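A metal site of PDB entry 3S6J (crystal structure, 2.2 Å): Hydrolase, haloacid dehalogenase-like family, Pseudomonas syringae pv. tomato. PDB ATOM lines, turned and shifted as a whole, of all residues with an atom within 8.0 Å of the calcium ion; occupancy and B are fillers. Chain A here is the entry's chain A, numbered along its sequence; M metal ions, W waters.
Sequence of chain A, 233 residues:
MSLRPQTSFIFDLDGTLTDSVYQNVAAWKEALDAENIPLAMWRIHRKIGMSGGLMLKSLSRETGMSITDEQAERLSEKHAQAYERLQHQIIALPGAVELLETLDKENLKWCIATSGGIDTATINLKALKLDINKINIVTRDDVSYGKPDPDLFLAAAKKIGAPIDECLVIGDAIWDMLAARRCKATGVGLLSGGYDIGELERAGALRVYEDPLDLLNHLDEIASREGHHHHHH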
ATOM      1  N   ASP A  12     -21.124  19.207  -9.815  1.00  0.00           N
ATOM      2  CA  ASP A  12     -20.773  20.254 -10.752  1.00  0.00           C
ATOM      3  C   ASP A  12     -19.660  19.692 -11.642  1.00  0.00           C
ATOM      4  O   ASP A  12     -18.958  18.717 -11.268  1.00  0.00           O
ATOM      5  CB  ASP A  12     -20.268  21.453  -9.974  1.00  0.00           C
ATOM      6  CG  ASP A  12     -19.721  22.526 -10.868  1.00  0.00           C
ATOM      7  OD1 ASP A  12     -20.451  23.111 -11.667  1.00  0.00           O
ATOM      8  OD2 ASP A  12     -18.539  22.801 -10.746  1.00  0.00           O
ATOM      9  N   LEU A  13     -19.476  20.279 -12.810  1.00  0.00           N
ATOM     10  CA  LEU A  13     -18.504  19.760 -13.772  1.00  0.00           C
ATOM     11  C   LEU A  13     -17.293  20.659 -13.898  1.00  0.00           C
ATOM     12  O   LEU A  13     -16.181  20.297 -13.557  1.00  0.00           O
ATOM     13  CB  LEU A  13     -19.171  19.597 -15.132  1.00  0.00           C
ATOM     14  CG  LEU A  13     -18.334  19.105 -16.309  1.00  0.00           C
ATOM     15  CD1 LEU A  13     -17.507  17.858 -15.910  1.00  0.00           C
ATOM     16  CD2 LEU A  13     -19.250  18.840 -17.567  1.00  0.00           C
ATOM     17  N   ASP A  14     -17.569  21.855 -14.406  1.00  0.00           N
ATOM     18  CA  ASP A  14     -16.578  22.877 -14.688  1.00  0.00           C
ATOM     19  C   ASP A  14     -15.918  23.399 -13.406  1.00  0.00           C
ATOM     20  O   ASP A  14     -16.502  24.232 -12.731  1.00  0.00           O
ATOM     21  CB  ASP A  14     -17.344  24.027 -15.409  1.00  0.00           C
ATOM     22  CG  ASP A  14     -16.495  25.272 -15.569  1.00  0.00           C
ATOM     23  OD1 ASP A  14     -15.270  25.133 -15.801  1.00  0.00           O
ATOM     24  OD2 ASP A  14     -17.046  26.384 -15.456  1.00  0.00           O
ATOM     25  N   GLY A  15     -14.716  22.931 -13.070  1.00  0.00           N
ATOM     26  CA  GLY A  15     -14.006  23.386 -11.872  1.00  0.00           C
ATOM     27  C   GLY A  15     -14.099  22.423 -10.682  1.00  0.00           C
ATOM     28  O   GLY A  15     -13.442  22.604  -9.653  1.00  0.00           O
ATOM     29  N   THR A  16     -14.934  21.405 -10.830  1.00  0.00           N
ATOM     30  CA  THR A  16     -15.199  20.444  -9.782  1.00  0.00           C
ATOM     31  C   THR A  16     -14.552  19.119 -10.176  1.00  0.00           C
ATOM     32  O   THR A  16     -13.819  18.544  -9.394  1.00  0.00           O
ATOM     33  CB  THR A  16     -16.725  20.274  -9.584  1.00  0.00           C
ATOM     34  OG1 THR A  16     -17.298  21.520  -9.143  1.00  0.00           O
ATOM     35  CG2 THR A  16     -17.040  19.176  -8.551  1.00  0.00           C
ATOM     36  N   LEU A  17     -14.814  18.671 -11.404  1.00  0.00           N
ATOM     37  CA  LEU A  17     -14.224  17.455 -11.956  1.00  0.00           C
ATOM     38  C   LEU A  17     -13.159  17.782 -13.016  1.00  0.00           C
ATOM     39  O   LEU A  17     -12.222  17.021 -13.208  1.00  0.00           O
ATOM     40  CB  LEU A  17     -15.307  16.571 -12.575  1.00  0.00           C
ATOM     41  CG  LEU A  17     -16.369  15.992 -11.647  1.00  0.00           C
ATOM     42  CD1 LEU A  17     -17.497  15.392 -12.462  1.00  0.00           C
ATOM     43  CD2 LEU A  17     -15.788  14.993 -10.629  1.00  0.00           C
ATOM     44  N   THR A  18     -13.345  18.888 -13.739  1.00  0.00           N
ATOM     45  CA  THR A  18     -12.348  19.353 -14.696  1.00  0.00           C
ATOM     46  C   THR A  18     -11.797  20.704 -14.270  1.00  0.00           C
ATOM     47  O   THR A  18     -12.495  21.489 -13.638  1.00  0.00           O
ATOM     48  CB  THR A  18     -12.918  19.474 -16.128  1.00  0.00           C
ATOM     49  OG1 THR A  18     -14.118  20.279 -16.128  1.00  0.00           O
ATOM     50  CG2 THR A  18     -13.218  18.068 -16.688  1.00  0.00           C
ATOM     51  N   SER A  20     -11.244  23.779 -15.482  1.00  0.00           N
ATOM     52  CA  SER A  20     -11.654  24.612 -16.614  1.00  0.00           C
ATOM     53  C   SER A  20     -12.166  25.980 -16.213  1.00  0.00           C
ATOM     54  O   SER A  20     -12.517  26.776 -17.090  1.00  0.00           O
ATOM     55  CB  SER A  20     -12.757  23.917 -17.415  1.00  0.00           C
ATOM     56  OG  SER A  20     -13.636  23.223 -16.552  1.00  0.00           O
ATOM     57  N   VAL A  21     -12.238  26.247 -14.903  1.00  0.00           N
ATOM     58  CA  VAL A  21     -12.760  27.546 -14.490  1.00  0.00           C
ATOM     59  C   VAL A  21     -11.928  28.696 -15.058  1.00  0.00           C
ATOM     60  O   VAL A  21     -12.457  29.685 -15.499  1.00  0.00           O
ATOM     61  CB  VAL A  21     -12.864  27.680 -12.970  1.00  0.00           C
ATOM     62  CG1 VAL A  21     -12.986  29.136 -12.581  1.00  0.00           C
ATOM     63  CG2 VAL A  21     -14.043  26.878 -12.445  1.00  0.00           C
ATOM     64  N   ASN A  24     -12.718  29.211 -18.621  1.00  0.00           N
ATOM     65  CA  ASN A  24     -14.039  29.802 -18.690  1.00  0.00           C
ATOM     66  C   ASN A  24     -13.956  31.304 -18.462  1.00  0.00           C
ATOM     67  O   ASN A  24     -14.520  32.079 -19.211  1.00  0.00           O
ATOM     68  CB  ASN A  24     -14.970  29.141 -17.681  1.00  0.00           C
ATOM     69  CG  ASN A  24     -16.398  29.245 -18.073  1.00  0.00           C
ATOM     70  OD1 ASN A  24     -16.801  30.163 -18.793  1.00  0.00           O
ATOM     71  ND2 ASN A  24     -17.203  28.302 -17.581  1.00  0.00           N
ATOM     72  N   LYS A  47     -18.353  34.948 -10.802  1.00  0.00           N
ATOM     73  CA  LYS A  47     -19.650  34.562 -11.362  1.00  0.00           C
ATOM     74  C   LYS A  47     -19.696  33.172 -12.008  1.00  0.00           C
ATOM     75  O   LYS A  47     -20.742  32.574 -12.148  1.00  0.00           O
ATOM     76  CB  LYS A  47     -20.146  35.640 -12.334  1.00  0.00           C
ATOM     77  CG  LYS A  47     -20.462  36.988 -11.678  1.00  0.00           C
ATOM     78  CD  LYS A  47     -21.086  36.804 -10.277  1.00  0.00           C
ATOM     79  CE  LYS A  47     -21.423  38.157  -9.633  1.00  0.00           C
ATOM     80  NZ  LYS A  47     -21.176  38.151  -8.151  1.00  0.00           N
ATOM     81  N   ILE A  48     -18.545  32.652 -12.411  1.00  0.00           N
ATOM     82  CA  ILE A  48     -18.518  31.368 -13.082  1.00  0.00           C
ATOM     83  C   ILE A  48     -19.288  30.335 -12.265  1.00  0.00           C
ATOM     84  O   ILE A  48     -19.005  30.108 -11.082  1.00  0.00           O
ATOM     85  CB  ILE A  48     -17.079  30.898 -13.334  1.00  0.00           C
ATOM     86  CG1 ILE A  48     -16.357  31.944 -14.189  1.00  0.00           C
ATOM     87  CG2 ILE A  48     -17.042  29.487 -13.978  1.00  0.00           C
ATOM     88  CD1 ILE A  48     -16.883  32.059 -15.628  1.00  0.00           C
ATOM     89  N   GLY A  49     -20.248  29.693 -12.918  1.00  0.00           N
ATOM     90  CA  GLY A  49     -21.164  28.792 -12.224  1.00  0.00           C
ATOM     91  C   GLY A  49     -22.616  29.245 -12.265  1.00  0.00           C
ATOM     92  O   GLY A  49     -23.513  28.432 -12.070  1.00  0.00           O
ATOM     93  N   MET A  50     -22.854  30.548 -12.489  1.00  0.00           N
ATOM     94  CA  MET A  50     -24.217  31.017 -12.770  1.00  0.00           C
ATOM     95  C   MET A  50     -24.533  30.713 -14.217  1.00  0.00           C
ATOM     96  O   MET A  50     -23.624  30.385 -14.990  1.00  0.00           O
ATOM     97  CB  MET A  50     -24.339  32.519 -12.569  1.00  0.00           C
ATOM     98  CG  MET A  50     -23.902  33.030 -11.217  1.00  0.00           C
ATOM     99  SD  MET A  50     -24.340  34.943 -10.985  1.00  0.00           S
ATOM    100  CE  MET A  50     -23.187  35.639 -12.343  1.00  0.00           C
ATOM    101  N   ALA A 113     -24.357  18.007 -13.185  1.00  0.00           N
ATOM    102  CA  ALA A 113     -25.326  19.073 -13.307  1.00  0.00           C
ATOM    103  C   ALA A 113     -24.564  20.369 -13.510  1.00  0.00           C
ATOM    104  O   ALA A 113     -23.901  20.847 -12.599  1.00  0.00           O
ATOM    105  CB  ALA A 113     -26.192  19.155 -12.032  1.00  0.00           C
ATOM    106  N   THR A 114     -24.675  20.945 -14.707  1.00  0.00           N
ATOM    107  CA  THR A 114     -23.882  22.130 -15.064  1.00  0.00           C
ATOM    108  C   THR A 114     -24.766  23.266 -15.561  1.00  0.00           C
ATOM    109  O   THR A 114     -25.810  23.004 -16.183  1.00  0.00           O
ATOM    110  CB  THR A 114     -22.779  21.797 -16.120  1.00  0.00           C
ATOM    111  OG1 THR A 114     -22.059  22.984 -16.453  1.00  0.00           O
ATOM    112  CG2 THR A 114     -23.380  21.169 -17.376  1.00  0.00           C
ATOM    113  N   SER A 115     -24.365  24.506 -15.288  1.00  0.00           N
ATOM    114  CA  SER A 115     -25.069  25.714 -15.775  1.00  0.00           C
ATOM    115  C   SER A 115     -24.738  26.004 -17.223  1.00  0.00           C
ATOM    116  O   SER A 115     -25.304  26.924 -17.814  1.00  0.00           O
ATOM    117  CB  SER A 115     -24.708  26.957 -14.947  1.00  0.00           C
ATOM    118  OG  SER A 115     -25.437  27.026 -13.739  1.00  0.00           O
ATOM    119  N   LYS A 147     -27.810  27.896 -11.938  1.00  0.00           N
ATOM    120  CA  LYS A 147     -27.485  28.204 -10.560  1.00  0.00           C
ATOM    121  C   LYS A 147     -27.445  29.711 -10.324  1.00  0.00           C
ATOM    122  O   LYS A 147     -27.097  30.467 -11.226  1.00  0.00           O
ATOM    123  CB  LYS A 147     -26.163  27.531 -10.204  1.00  0.00           C
ATOM    124  CG  LYS A 147     -26.113  26.099 -10.664  1.00  0.00           C
ATOM    125  CD  LYS A 147     -24.771  25.468 -10.361  1.00  0.00           C
ATOM    126  CE  LYS A 147     -24.528  24.263 -11.290  1.00  0.00           C
ATOM    127  NZ  LYS A 147     -23.245  23.576 -10.987  1.00  0.00           N
ATOM    128  N   ILE A 170     -21.849  18.313  -4.899  1.00  0.00           N
ATOM    129  CA  ILE A 170     -20.420  18.576  -4.896  1.00  0.00           C
ATOM    130  C   ILE A 170     -20.103  19.655  -5.916  1.00  0.00           C
ATOM    131  O   ILE A 170     -20.246  19.439  -7.112  1.00  0.00           O
ATOM    132  CB  ILE A 170     -19.586  17.305  -5.157  1.00  0.00           C
ATOM    133  CG1 ILE A 170     -19.821  16.300  -4.034  1.00  0.00           C
ATOM    134  CG2 ILE A 170     -18.081  17.661  -5.222  1.00  0.00           C
ATOM    135  CD1 ILE A 170     -19.220  14.953  -4.245  1.00  0.00           C
ATOM    136  N   GLY A 171     -19.704  20.820  -5.425  1.00  0.00           N
ATOM    137  CA  GLY A 171     -19.407  21.941  -6.299  1.00  0.00           C
ATOM    138  C   GLY A 171     -18.215  22.729  -5.832  1.00  0.00           C
ATOM    139  O   GLY A 171     -17.692  22.517  -4.727  1.00  0.00           O
ATOM    140  N   ASP A 172     -17.791  23.668  -6.669  1.00  0.00           N
ATOM    141  CA  ASP A 172     -16.600  24.438  -6.398  1.00  0.00           C
ATOM    142  C   ASP A 172     -16.966  25.897  -6.201  1.00  0.00           C
ATOM    143  O   ASP A 172     -16.125  26.705  -5.825  1.00  0.00           O
ATOM    144  CB  ASP A 172     -15.673  24.370  -7.591  1.00  0.00           C
ATOM    145  CG  ASP A 172     -16.326  24.938  -8.837  1.00  0.00           C
ATOM    146  OD1 ASP A 172     -17.571  24.871  -8.905  1.00  0.00           O
ATOM    147  OD2 ASP A 172     -15.633  25.508  -9.698  1.00  0.00           O
ATOM    148  N   ALA A 173     -18.216  26.241  -6.495  1.00  0.00           N
ATOM    149  CA  ALA A 173     -18.585  27.645  -6.481  1.00  0.00           C
ATOM    150  C   ALA A 173     -19.625  27.969  -5.419  1.00  0.00           C
ATOM    151  O   ALA A 173     -20.371  27.112  -4.956  1.00  0.00           O
ATOM    152  CB  ALA A 173     -19.049  28.115  -7.890  1.00  0.00           C
ATOM    153  N   ILE A 174     -19.660  29.228  -5.047  1.00  0.00           N
ATOM    154  CA  ILE A 174     -20.670  29.763  -4.167  1.00  0.00           C
ATOM    155  C   ILE A 174     -22.082  29.443  -4.705  1.00  0.00           C
ATOM    156  O   ILE A 174     -22.972  29.062  -3.939  1.00  0.00           O
ATOM    157  CB  ILE A 174     -20.371  31.250  -3.992  1.00  0.00           C
ATOM    158  CG1 ILE A 174     -19.542  31.466  -2.711  1.00  0.00           C
ATOM    159  CG2 ILE A 174     -21.596  32.144  -4.096  1.00  0.00           C
ATOM    160  CD1 ILE A 174     -19.293  32.937  -2.423  1.00  0.00           C
ATOM    161  N   TRP A 175     -22.270  29.548  -6.012  1.00  0.00           N
ATOM    162  CA  TRP A 175     -23.562  29.256  -6.666  1.00  0.00           C
ATOM    163  C   TRP A 175     -24.033  27.811  -6.518  1.00  0.00           C
ATOM    164  O   TRP A 175     -25.221  27.557  -6.383  1.00  0.00           O
ATOM    165  CB  TRP A 175     -23.497  29.675  -8.140  1.00  0.00           C
ATOM    166  CG  TRP A 175     -22.788  30.975  -8.242  1.00  0.00           C
ATOM    167  CD1 TRP A 175     -21.589  31.210  -8.838  1.00  0.00           C
ATOM    168  CD2 TRP A 175     -23.192  32.208  -7.643  1.00  0.00           C
ATOM    169  NE1 TRP A 175     -21.232  32.527  -8.668  1.00  0.00           N
ATOM    170  CE2 TRP A 175     -22.205  33.164  -7.932  1.00  0.00           C
ATOM    171  CE3 TRP A 175     -24.311  32.597  -6.894  1.00  0.00           C
ATOM    172  CZ2 TRP A 175     -22.295  34.492  -7.513  1.00  0.00           C
ATOM    173  CZ3 TRP A 175     -24.405  33.915  -6.458  1.00  0.00           C
ATOM    174  CH2 TRP A 175     -23.394  34.847  -6.771  1.00  0.00           C
ATOM    175  N   ASP A 176     -23.091  26.859  -6.520  1.00  0.00           N
ATOM    176  CA  ASP A 176     -23.403  25.469  -6.231  1.00  0.00           C
ATOM    177  C   ASP A 176     -23.926  25.336  -4.813  1.00  0.00           C
ATOM    178  O   ASP A 176     -24.948  24.693  -4.577  1.00  0.00           O
ATOM    179  CB  ASP A 176     -22.168  24.564  -6.400  1.00  0.00           C
ATOM    180  CG  ASP A 176     -21.634  24.598  -7.821  1.00  0.00           C
ATOM    181  OD1 ASP A 176     -22.266  24.017  -8.723  1.00  0.00           O
ATOM    182  OD2 ASP A 176     -20.581  25.221  -8.028  1.00  0.00           O
ATOM    183  N   SER A 192     -10.946  23.750  -5.975  1.00  0.00           N
ATOM    184  CA  SER A 192     -10.309  23.602  -7.290  1.00  0.00           C
ATOM    185  C   SER A 192     -10.904  24.544  -8.324  1.00  0.00           C
ATOM    186  O   SER A 192     -10.489  24.564  -9.497  1.00  0.00           O
ATOM    187  CB  SER A 192     -10.427  22.143  -7.728  1.00  0.00           C
ATOM    188  OG  SER A 192     -11.788  21.725  -7.700  1.00  0.00           O
ATOM    189  N   GLY A 193     -11.888  25.338  -7.900  1.00  0.00           N
ATOM    190  CA  GLY A 193     -12.512  26.324  -8.775  1.00  0.00           C
ATOM    191  C   GLY A 193     -11.963  27.711  -8.473  1.00  0.00           C
ATOM    192  O   GLY A 193     -12.350  28.697  -9.095  1.00  0.00           O
ATOM    193  N   TYR A 195     -12.492  29.334  -5.614  1.00  0.00           N
ATOM    194  CA  TYR A 195     -13.188  29.997  -4.489  1.00  0.00           C
ATOM    195  C   TYR A 195     -12.508  29.620  -3.159  1.00  0.00           C
ATOM    196  O   TYR A 195     -11.953  28.514  -3.047  1.00  0.00           O
ATOM    197  CB  TYR A 195     -14.693  29.641  -4.473  1.00  0.00           C
ATOM    198  CG  TYR A 195     -15.546  30.232  -5.633  1.00  0.00           C
ATOM    199  CD1 TYR A 195     -15.461  29.711  -6.904  1.00  0.00           C
ATOM    200  CD2 TYR A 195     -16.426  31.295  -5.423  1.00  0.00           C
ATOM    201  CE1 TYR A 195     -16.214  30.217  -7.967  1.00  0.00           C
ATOM    202  CE2 TYR A 195     -17.223  31.830  -6.500  1.00  0.00           C
ATOM    203  CZ  TYR A 195     -17.092  31.261  -7.769  1.00  0.00           C
ATOM    204  OH  TYR A 195     -17.811  31.698  -8.885  1.00  0.00           O
HETATM  205 CA    CA M   1     -18.161  25.228 -11.353  1.00  0.00          CA
HETATM  206  O   HOH W   1     -17.212  27.487 -11.205  1.00  0.00           O
HETATM  207  O   HOH W   2     -20.398  25.846 -10.523  1.00  0.00           O
HETATM  208  O   HOH W   3     -19.148  26.265 -13.521  1.00  0.00           O
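The backbone NH (N) of Val 21 sits at hydrogen-bond distance from the side-chain carboxylate (OD1) of Asp 14, 3.4 Å away.
The side-chain amide nitrogen (ND2) of Asn 24 is in hydrogen-bond range of the side-chain carboxylate (OD2) of Asp 14.
The side-chain hydroxyl (OG) of Ser 20 lies within hydrogen-bond range of the side-chain carboxylate (OD1) of Asp 14 (2.6 Å).
OD1 of Asp 12 is in salt-bridge range of NZ of Lys 147.
The backbone NH (N) of Asp 12 lies within hydrogen-bond range of the backbone carbonyl oxygen (O) of Ile 170, 2.9 Å away.
The backbone NH of Asp 172 lies within hydrogen-bond range of the side-chain carboxylate of Asp 176 (3.5 Å).
OG1 of Thr 16 lies within hydrogen-bond range of N of Asp 172 (3.3 Å).
Water W1 lies within hydrogen-bond range of the side-chain carboxylate (OD2) of Asp 172 and the backbone carbonyl oxygen (O) of Ile 48.
Water W2 bridges OD2 of Asp 176 (2.6 Å) and OD1 of Asp 12 (3.0 Å).
The nearest printed residue that does not touch the calcium ion is Asp 176 (4.1 Å).
The calcium ion is bound by the backbone carbonyl oxygen of Asp 14, water W1, water W2, the side-chain carboxylate of Asp 12, the side-chain carboxylate of Asp 172 and water W3.
Slightly farther from the calcium ion lies the side-chain carboxylate (OD2) of Asp 172 (3.0 Å).
Slightly farther from the calcium ion lies the side-chain carboxylate (OD1) of Asp 12 (3.1 Å).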
